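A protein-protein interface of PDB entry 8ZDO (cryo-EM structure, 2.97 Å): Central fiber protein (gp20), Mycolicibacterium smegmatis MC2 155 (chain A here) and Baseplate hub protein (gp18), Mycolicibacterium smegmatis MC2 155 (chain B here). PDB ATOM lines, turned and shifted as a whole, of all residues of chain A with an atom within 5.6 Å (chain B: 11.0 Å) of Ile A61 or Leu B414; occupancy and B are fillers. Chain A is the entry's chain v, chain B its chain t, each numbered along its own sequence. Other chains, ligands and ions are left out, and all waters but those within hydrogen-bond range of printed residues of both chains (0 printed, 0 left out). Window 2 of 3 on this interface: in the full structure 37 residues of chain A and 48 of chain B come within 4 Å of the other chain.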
ATOM      1  N   ALA A  53      25.435   3.397  32.951  1.00  0.00           N
ATOM      2  CA  ALA A  53      26.253   3.391  31.744  1.00  0.00           C
ATOM      3  C   ALA A  53      27.550   4.160  31.959  1.00  0.00           C
ATOM      4  O   ALA A  53      28.609   3.749  31.478  1.00  0.00           O
ATOM      5  CB  ALA A  53      25.468   3.975  30.573  1.00  0.00           C
ATOM      6  N   SER A  54      27.481   5.285  32.675  1.00  0.00           N
ATOM      7  CA  SER A  54      28.688   6.043  32.985  1.00  0.00           C
ATOM      8  C   SER A  54      29.647   5.227  33.836  1.00  0.00           C
ATOM      9  O   SER A  54      30.859   5.223  33.592  1.00  0.00           O
ATOM     10  CB  SER A  54      28.317   7.344  33.693  1.00  0.00           C
ATOM     11  OG  SER A  54      29.475   8.068  34.065  1.00  0.00           O
ATOM     12  N   THR A  56      29.863   1.943  33.953  1.00  0.00           N
ATOM     13  CA  THR A  56      30.418   0.887  33.114  1.00  0.00           C
ATOM     14  C   THR A  56      31.487   1.428  32.173  1.00  0.00           C
ATOM     15  O   THR A  56      32.537   0.803  31.988  1.00  0.00           O
ATOM     16  CB  THR A  56      29.303   0.209  32.320  1.00  0.00           C
ATOM     17  OG1 THR A  56      28.330  -0.328  33.225  1.00  0.00           O
ATOM     18  CG2 THR A  56      29.863  -0.912  31.465  1.00  0.00           C
ATOM     19  N   PHE A  57      31.238   2.589  31.570  1.00  0.00           N
ATOM     20  CA  PHE A  57      32.178   3.143  30.604  1.00  0.00           C
ATOM     21  C   PHE A  57      33.469   3.588  31.275  1.00  0.00           C
ATOM     22  O   PHE A  57      34.566   3.246  30.819  1.00  0.00           O
ATOM     23  CB  PHE A  57      31.532   4.309  29.859  1.00  0.00           C
ATOM     24  CG  PHE A  57      32.418   4.933  28.823  1.00  0.00           C
ATOM     25  CD1 PHE A  57      32.758   4.242  27.677  1.00  0.00           C
ATOM     26  CD2 PHE A  57      32.908   6.213  28.996  1.00  0.00           C
ATOM     27  CE1 PHE A  57      33.571   4.817  26.724  1.00  0.00           C
ATOM     28  CE2 PHE A  57      33.720   6.792  28.047  1.00  0.00           C
ATOM     29  CZ  PHE A  57      34.052   6.092  26.910  1.00  0.00           C
ATOM     30  N   PHE A  58      33.364   4.345  32.366  1.00  0.00           N
ATOM     31  CA  PHE A  58      34.540   4.962  32.960  1.00  0.00           C
ATOM     32  C   PHE A  58      35.295   4.049  33.913  1.00  0.00           C
ATOM     33  O   PHE A  58      36.488   4.273  34.137  1.00  0.00           O
ATOM     34  CB  PHE A  58      34.145   6.247  33.689  1.00  0.00           C
ATOM     35  CG  PHE A  58      33.717   7.348  32.770  1.00  0.00           C
ATOM     36  CD1 PHE A  58      34.611   7.899  31.872  1.00  0.00           C
ATOM     37  CD2 PHE A  58      32.419   7.822  32.791  1.00  0.00           C
ATOM     38  CE1 PHE A  58      34.220   8.907  31.018  1.00  0.00           C
ATOM     39  CE2 PHE A  58      32.024   8.830  31.938  1.00  0.00           C
ATOM     40  CZ  PHE A  58      32.926   9.372  31.053  1.00  0.00           C
ATOM     41  N   ASN A  59      34.647   3.031  34.477  1.00  0.00           N
ATOM     42  CA  ASN A  59      35.303   2.134  35.419  1.00  0.00           C
ATOM     43  C   ASN A  59      35.678   0.799  34.792  1.00  0.00           C
ATOM     44  O   ASN A  59      36.804   0.328  34.966  1.00  0.00           O
ATOM     45  CB  ASN A  59      34.401   1.905  36.637  1.00  0.00           C
ATOM     46  CG  ASN A  59      34.111   3.182  37.394  1.00  0.00           C
ATOM     47  OD1 ASN A  59      35.023   3.941  37.723  1.00  0.00           O
ATOM     48  ND2 ASN A  59      32.838   3.429  37.674  1.00  0.00           N
ATOM     49  N   LEU A  60      34.758   0.178  34.056  1.00  0.00           N
ATOM     50  CA  LEU A  60      35.051  -1.111  33.440  1.00  0.00           C
ATOM     51  C   LEU A  60      35.815  -0.943  32.131  1.00  0.00           C
ATOM     52  O   LEU A  60      36.944  -1.423  31.993  1.00  0.00           O
ATOM     53  CB  LEU A  60      33.754  -1.893  33.215  1.00  0.00           C
ATOM     54  CG  LEU A  60      33.825  -3.075  32.248  1.00  0.00           C
ATOM     55  CD1 LEU A  60      34.623  -4.216  32.854  1.00  0.00           C
ATOM     56  CD2 LEU A  60      32.431  -3.536  31.870  1.00  0.00           C
ATOM     57  N   ILE A  61      35.212  -0.252  31.161  1.00  0.00           N
ATOM     58  CA  ILE A  61      35.806  -0.166  29.830  1.00  0.00           C
ATOM     59  C   ILE A  61      37.101   0.634  29.861  1.00  0.00           C
ATOM     60  O   ILE A  61      38.102   0.245  29.248  1.00  0.00           O
ATOM     61  CB  ILE A  61      34.796   0.431  28.834  1.00  0.00           C
ATOM     62  CG1 ILE A  61      33.632  -0.534  28.628  1.00  0.00           C
ATOM     63  CG2 ILE A  61      35.467   0.735  27.510  1.00  0.00           C
ATOM     64  CD1 ILE A  61      32.563  -0.001  27.723  1.00  0.00           C
ATOM     65  N   LEU A  62      37.111   1.757  30.573  1.00  0.00           N
ATOM     66  CA  LEU A  62      38.267   2.639  30.610  1.00  0.00           C
ATOM     67  C   LEU A  62      39.182   2.371  31.797  1.00  0.00           C
ATOM     68  O   LEU A  62      40.131   3.129  32.011  1.00  0.00           O
ATOM     69  CB  LEU A  62      37.815   4.100  30.629  1.00  0.00           C
ATOM     70  CG  LEU A  62      37.365   4.683  29.290  1.00  0.00           C
ATOM     71  CD1 LEU A  62      36.928   6.121  29.464  1.00  0.00           C
ATOM     72  CD2 LEU A  62      38.475   4.583  28.263  1.00  0.00           C
ATOM     73  N   GLY A  63      38.927   1.313  32.563  1.00  0.00           N
ATOM     74  CA  GLY A  63      39.744   1.050  33.737  1.00  0.00           C
ATOM     75  C   GLY A  63      39.576   2.146  34.771  1.00  0.00           C
ATOM     76  O   GLY A  63      38.471   2.636  35.021  1.00  0.00           O
ATOM     77  N   THR B 405      15.261   5.260  27.961  1.00  0.00           N
ATOM     78  CA  THR B 405      15.502   4.156  27.042  1.00  0.00           C
ATOM     79  C   THR B 405      16.860   4.276  26.367  1.00  0.00           C
ATOM     80  O   THR B 405      17.554   3.270  26.197  1.00  0.00           O
ATOM     81  CB  THR B 405      14.394   4.076  25.999  1.00  0.00           C
ATOM     82  OG1 THR B 405      14.497   5.191  25.108  1.00  0.00           O
ATOM     83  CG2 THR B 405      13.041   4.092  26.677  1.00  0.00           C
ATOM     84  N   THR B 406      17.273   5.488  25.981  1.00  0.00           N
ATOM     85  CA  THR B 406      18.590   5.610  25.369  1.00  0.00           C
ATOM     86  C   THR B 406      19.696   5.352  26.385  1.00  0.00           C
ATOM     87  O   THR B 406      20.726   4.767  26.036  1.00  0.00           O
ATOM     88  CB  THR B 406      18.749   6.975  24.690  1.00  0.00           C
ATOM     89  OG1 THR B 406      19.868   6.936  23.800  1.00  0.00           O
ATOM     90  CG2 THR B 406      18.957   8.086  25.698  1.00  0.00           C
ATOM     91  N   GLY B 407      19.487   5.725  27.650  1.00  0.00           N
ATOM     92  CA  GLY B 407      20.468   5.393  28.669  1.00  0.00           C
ATOM     93  C   GLY B 407      20.570   3.901  28.914  1.00  0.00           C
ATOM     94  O   GLY B 407      21.672   3.358  29.038  1.00  0.00           O
ATOM     95  N   ASN B 408      19.426   3.218  28.989  1.00  0.00           N
ATOM     96  CA  ASN B 408      19.434   1.772  29.177  1.00  0.00           C
ATOM     97  C   ASN B 408      20.078   1.066  27.990  1.00  0.00           C
ATOM     98  O   ASN B 408      20.842   0.111  28.164  1.00  0.00           O
ATOM     99  CB  ASN B 408      18.011   1.266  29.395  1.00  0.00           C
ATOM    100  CG  ASN B 408      17.408   1.774  30.684  1.00  0.00           C
ATOM    101  OD1 ASN B 408      18.115   2.013  31.660  1.00  0.00           O
ATOM    102  ND2 ASN B 408      16.092   1.945  30.693  1.00  0.00           N
ATOM    103  N   LEU B 409      19.775   1.523  26.773  1.00  0.00           N
ATOM    104  CA  LEU B 409      20.389   0.941  25.586  1.00  0.00           C
ATOM    105  C   LEU B 409      21.894   1.162  25.580  1.00  0.00           C
ATOM    106  O   LEU B 409      22.654   0.261  25.215  1.00  0.00           O
ATOM    107  CB  LEU B 409      19.757   1.525  24.326  1.00  0.00           C
ATOM    108  CG  LEU B 409      18.424   0.914  23.900  1.00  0.00           C
ATOM    109  CD1 LEU B 409      17.680   1.857  22.974  1.00  0.00           C
ATOM    110  CD2 LEU B 409      18.651  -0.427  23.236  1.00  0.00           C
ATOM    111  N   LEU B 410      22.347   2.353  25.975  1.00  0.00           N
ATOM    112  CA  LEU B 410      23.783   2.601  26.026  1.00  0.00           C
ATOM    113  C   LEU B 410      24.458   1.742  27.086  1.00  0.00           C
ATOM    114  O   LEU B 410      25.572   1.255  26.875  1.00  0.00           O
ATOM    115  CB  LEU B 410      24.061   4.079  26.281  1.00  0.00           C
ATOM    116  CG  LEU B 410      25.513   4.474  26.015  1.00  0.00           C
ATOM    117  CD1 LEU B 410      25.869   4.245  24.557  1.00  0.00           C
ATOM    118  CD2 LEU B 410      25.764   5.909  26.406  1.00  0.00           C
ATOM    119  N   GLY B 411      23.810   1.555  28.238  1.00  0.00           N
ATOM    120  CA  GLY B 411      24.371   0.672  29.250  1.00  0.00           C
ATOM    121  C   GLY B 411      24.472  -0.764  28.774  1.00  0.00           C
ATOM    122  O   GLY B 411      25.489  -1.430  28.986  1.00  0.00           O
ATOM    123  N   TYR B 412      23.424  -1.252  28.107  1.00  0.00           N
ATOM    124  CA  TYR B 412      23.447  -2.591  27.528  1.00  0.00           C
ATOM    125  C   TYR B 412      24.554  -2.720  26.489  1.00  0.00           C
ATOM    126  O   TYR B 412      25.283  -3.718  26.458  1.00  0.00           O
ATOM    127  CB  TYR B 412      22.082  -2.886  26.906  1.00  0.00           C
ATOM    128  CG  TYR B 412      21.826  -4.322  26.528  1.00  0.00           C
ATOM    129  CD1 TYR B 412      21.853  -5.326  27.480  1.00  0.00           C
ATOM    130  CD2 TYR B 412      21.527  -4.668  25.217  1.00  0.00           C
ATOM    131  CE1 TYR B 412      21.606  -6.637  27.135  1.00  0.00           C
ATOM    132  CE2 TYR B 412      21.280  -5.974  24.864  1.00  0.00           C
ATOM    133  CZ  TYR B 412      21.321  -6.955  25.828  1.00  0.00           C
ATOM    134  OH  TYR B 412      21.076  -8.262  25.484  1.00  0.00           O
ATOM    135  N   PHE B 413      24.701  -1.702  25.642  1.00  0.00           N
ATOM    136  CA  PHE B 413      25.732  -1.698  24.610  1.00  0.00           C
ATOM    137  C   PHE B 413      27.130  -1.719  25.217  1.00  0.00           C
ATOM    138  O   PHE B 413      28.002  -2.470  24.766  1.00  0.00           O
ATOM    139  CB  PHE B 413      25.526  -0.474  23.717  1.00  0.00           C
ATOM    140  CG  PHE B 413      26.748  -0.039  22.974  1.00  0.00           C
ATOM    141  CD1 PHE B 413      27.066  -0.592  21.753  1.00  0.00           C
ATOM    142  CD2 PHE B 413      27.560   0.958  23.484  1.00  0.00           C
ATOM    143  CE1 PHE B 413      28.184  -0.179  21.070  1.00  0.00           C
ATOM    144  CE2 PHE B 413      28.678   1.370  22.805  1.00  0.00           C
ATOM    145  CZ  PHE B 413      28.989   0.802  21.596  1.00  0.00           C
ATOM    146  N   LEU B 414      27.363  -0.902  26.245  1.00  0.00           N
ATOM    147  CA  LEU B 414      28.680  -0.867  26.869  1.00  0.00           C
ATOM    148  C   LEU B 414      28.972  -2.154  27.626  1.00  0.00           C
ATOM    149  O   LEU B 414      30.134  -2.564  27.722  1.00  0.00           O
ATOM    150  CB  LEU B 414      28.793   0.339  27.802  1.00  0.00           C
ATOM    151  CG  LEU B 414      28.718   1.716  27.139  1.00  0.00           C
ATOM    152  CD1 LEU B 414      28.598   2.807  28.183  1.00  0.00           C
ATOM    153  CD2 LEU B 414      29.916   1.961  26.244  1.00  0.00           C
ATOM    154  N   LEU B 415      27.941  -2.803  28.173  1.00  0.00           N
ATOM    155  CA  LEU B 415      28.141  -4.118  28.768  1.00  0.00           C
ATOM    156  C   LEU B 415      28.361  -5.193  27.714  1.00  0.00           C
ATOM    157  O   LEU B 415      28.924  -6.246  28.027  1.00  0.00           O
ATOM    158  CB  LEU B 415      26.950  -4.486  29.650  1.00  0.00           C
ATOM    159  CG  LEU B 415      26.919  -3.811  31.020  1.00  0.00           C
ATOM    160  CD1 LEU B 415      25.660  -4.187  31.779  1.00  0.00           C
ATOM    161  CD2 LEU B 415      28.158  -4.178  31.815  1.00  0.00           C
ATOM    162  N   GLY B 416      27.934  -4.954  26.482  1.00  0.00           N
ATOM    163  CA  GLY B 416      28.153  -5.882  25.399  1.00  0.00           C
ATOM    164  C   GLY B 416      26.967  -6.738  25.029  1.00  0.00           C
ATOM    165  O   GLY B 416      27.164  -7.843  24.514  1.00  0.00           O
ATOM    166  N   GLY B 417      25.744  -6.269  25.276  1.00  0.00           N
ATOM    167  CA  GLY B 417      24.579  -7.081  24.974  1.00  0.00           C
ATOM    168  C   GLY B 417      24.398  -7.329  23.490  1.00  0.00           C
ATOM    169  O   GLY B 417      23.987  -8.417  23.080  1.00  0.00           O
ATOM    170  N   PHE B 418      24.697  -6.328  22.664  1.00  0.00           N
ATOM    171  CA  PHE B 418      24.551  -6.487  21.226  1.00  0.00           C
ATOM    172  C   PHE B 418      25.693  -7.274  20.603  1.00  0.00           C
ATOM    173  O   PHE B 418      25.555  -7.753  19.474  1.00  0.00           O
ATOM    174  CB  PHE B 418      24.424  -5.115  20.568  1.00  0.00           C
ATOM    175  CG  PHE B 418      23.234  -4.340  21.035  1.00  0.00           C
ATOM    176  CD1 PHE B 418      21.976  -4.612  20.531  1.00  0.00           C
ATOM    177  CD2 PHE B 418      23.366  -3.351  21.995  1.00  0.00           C
ATOM    178  CE1 PHE B 418      20.878  -3.907  20.966  1.00  0.00           C
ATOM    179  CE2 PHE B 418      22.270  -2.643  22.433  1.00  0.00           C
ATOM    180  CZ  PHE B 418      21.025  -2.919  21.917  1.00  0.00           C
ATOM    181  N   SER B 419      26.816  -7.413  21.309  1.00  0.00           N
ATOM    182  CA  SER B 419      27.872  -8.301  20.838  1.00  0.00           C
ATOM    183  C   SER B 419      27.490  -9.760  21.052  1.00  0.00           C
ATOM    184  O   SER B 419      27.738 -10.607  20.187  1.00  0.00           O
ATOM    185  CB  SER B 419      29.184  -7.974  21.549  1.00  0.00           C
ATOM    186  OG  SER B 419      30.249  -8.762  21.048  1.00  0.00           O
ATOM    187  N   SER B 420      26.885 -10.068  22.197  1.00  0.00           N
ATOM    188  CA  SER B 420      26.397 -11.406  22.494  1.00  0.00           C
ATOM    189  C   SER B 420      25.243 -11.293  23.479  1.00  0.00           C
ATOM    190  O   SER B 420      25.288 -10.478  24.405  1.00  0.00           O
ATOM    191  CB  SER B 420      27.504 -12.298  23.064  1.00  0.00           C
ATOM    192  OG  SER B 420      27.955 -11.813  24.316  1.00  0.00           O
ATOM    193  N   THR B 423      24.125 -10.778  28.160  1.00  0.00           N
ATOM    194  CA  THR B 423      23.821  -9.717  29.109  1.00  0.00           C
ATOM    195  C   THR B 423      22.315  -9.609  29.346  1.00  0.00           C
ATOM    196  O   THR B 423      21.504  -9.794  28.436  1.00  0.00           O
ATOM    197  CB  THR B 423      24.375  -8.382  28.605  1.00  0.00           C
ATOM    198  OG1 THR B 423      25.788  -8.499  28.398  1.00  0.00           O
ATOM    199  CG2 THR B 423      24.126  -7.271  29.613  1.00  0.00           C
ATOM    200  N   ILE B 424      21.949  -9.309  30.590  1.00  0.00           N
ATOM    201  CA  ILE B 424      20.559  -9.106  30.983  1.00  0.00           C
ATOM    202  C   ILE B 424      20.248  -7.620  30.875  1.00  0.00           C
ATOM    203  O   ILE B 424      20.923  -6.790  31.496  1.00  0.00           O
ATOM    204  CB  ILE B 424      20.294  -9.622  32.406  1.00  0.00           C
ATOM    205  CG1 ILE B 424      20.588 -11.121  32.495  1.00  0.00           C
ATOM    206  CG2 ILE B 424      18.862  -9.325  32.821  1.00  0.00           C
ATOM    207  CD1 ILE B 424      19.709 -11.969  31.604  1.00  0.00           C
ATOM    208  N   ALA B 425      19.226  -7.284  30.095  1.00  0.00           N
ATOM    209  CA  ALA B 425      18.880  -5.892  29.854  1.00  0.00           C
ATOM    210  C   ALA B 425      17.981  -5.354  30.963  1.00  0.00           C
ATOM    211  O   ALA B 425      17.413  -6.103  31.762  1.00  0.00           O
ATOM    212  CB  ALA B 425      18.188  -5.739  28.502  1.00  0.00           C
ATOM    213  N   ILE B 428      14.891  -1.950  27.967  1.00  0.00           N
ATOM    214  CA  ILE B 428      15.295  -1.394  26.683  1.00  0.00           C
ATOM    215  C   ILE B 428      14.182  -1.498  25.647  1.00  0.00           C
ATOM    216  O   ILE B 428      14.413  -1.238  24.464  1.00  0.00           O
ATOM    217  CB  ILE B 428      16.578  -2.063  26.169  1.00  0.00           C
ATOM    218  CG1 ILE B 428      16.341  -3.556  25.946  1.00  0.00           C
ATOM    219  CG2 ILE B 428      17.716  -1.844  27.148  1.00  0.00           C
ATOM    220  CD1 ILE B 428      17.513  -4.270  25.320  1.00  0.00           C
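The backbone carbonyl oxygen (O) of Phe A57 is in hydrogen-bond range of the backbone NH (N) of Leu A62 (3.0 Å).
N of Ile A61 is in hydrogen-bond range of O of Thr A56 (3.0 Å).
Among the printed residues, pairs that only touch across the chains: Ala A53 with Leu B414 (3.4 Å), Ile A61 with Leu B414 (3.5 Å), Phe A57 with Leu B414 (3.7 Å), Thr A56 with Leu B415 (3.7 Å) and Ala A53 with Gly B411 (3.7 Å).
Of chain B, only Leu B414 (3.5 Å) comes within 4 Å of Ile A61.
Of the printed residues of chain B, Ala A53 touches Gly B411 and Leu B414.
Phe A57 touches just one residue of chain B: Leu B414.
Leu A62 touches none of the printed residues of chain B.
Printed residues of chain A within 4 Å of Gly B411: Ala A53.
Printed residues of chain B within 4 Å of Thr A56: Leu B415.
Printed residues of chain A within 4 Å of Leu B415: Thr A56 (3.7 Å).
The nearest printed residue of chain A that does not touch Leu B414 is Thr A56 (4.02 Å).
The nearest printed residue of chain B that does not touch Thr A56 is Leu B414 (4.02 Å).
Of the 20 printed residues of chain B, 3 touch a printed residue of chain A.
Hydrophobic or aromatic side chains of chain B that line the printed part of chain A: Leu B414 and Leu B415.
Hydrophobic or aromatic side chains of chain A that line the printed part of chain B: Ala A53, Phe A57 and Ile A61.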
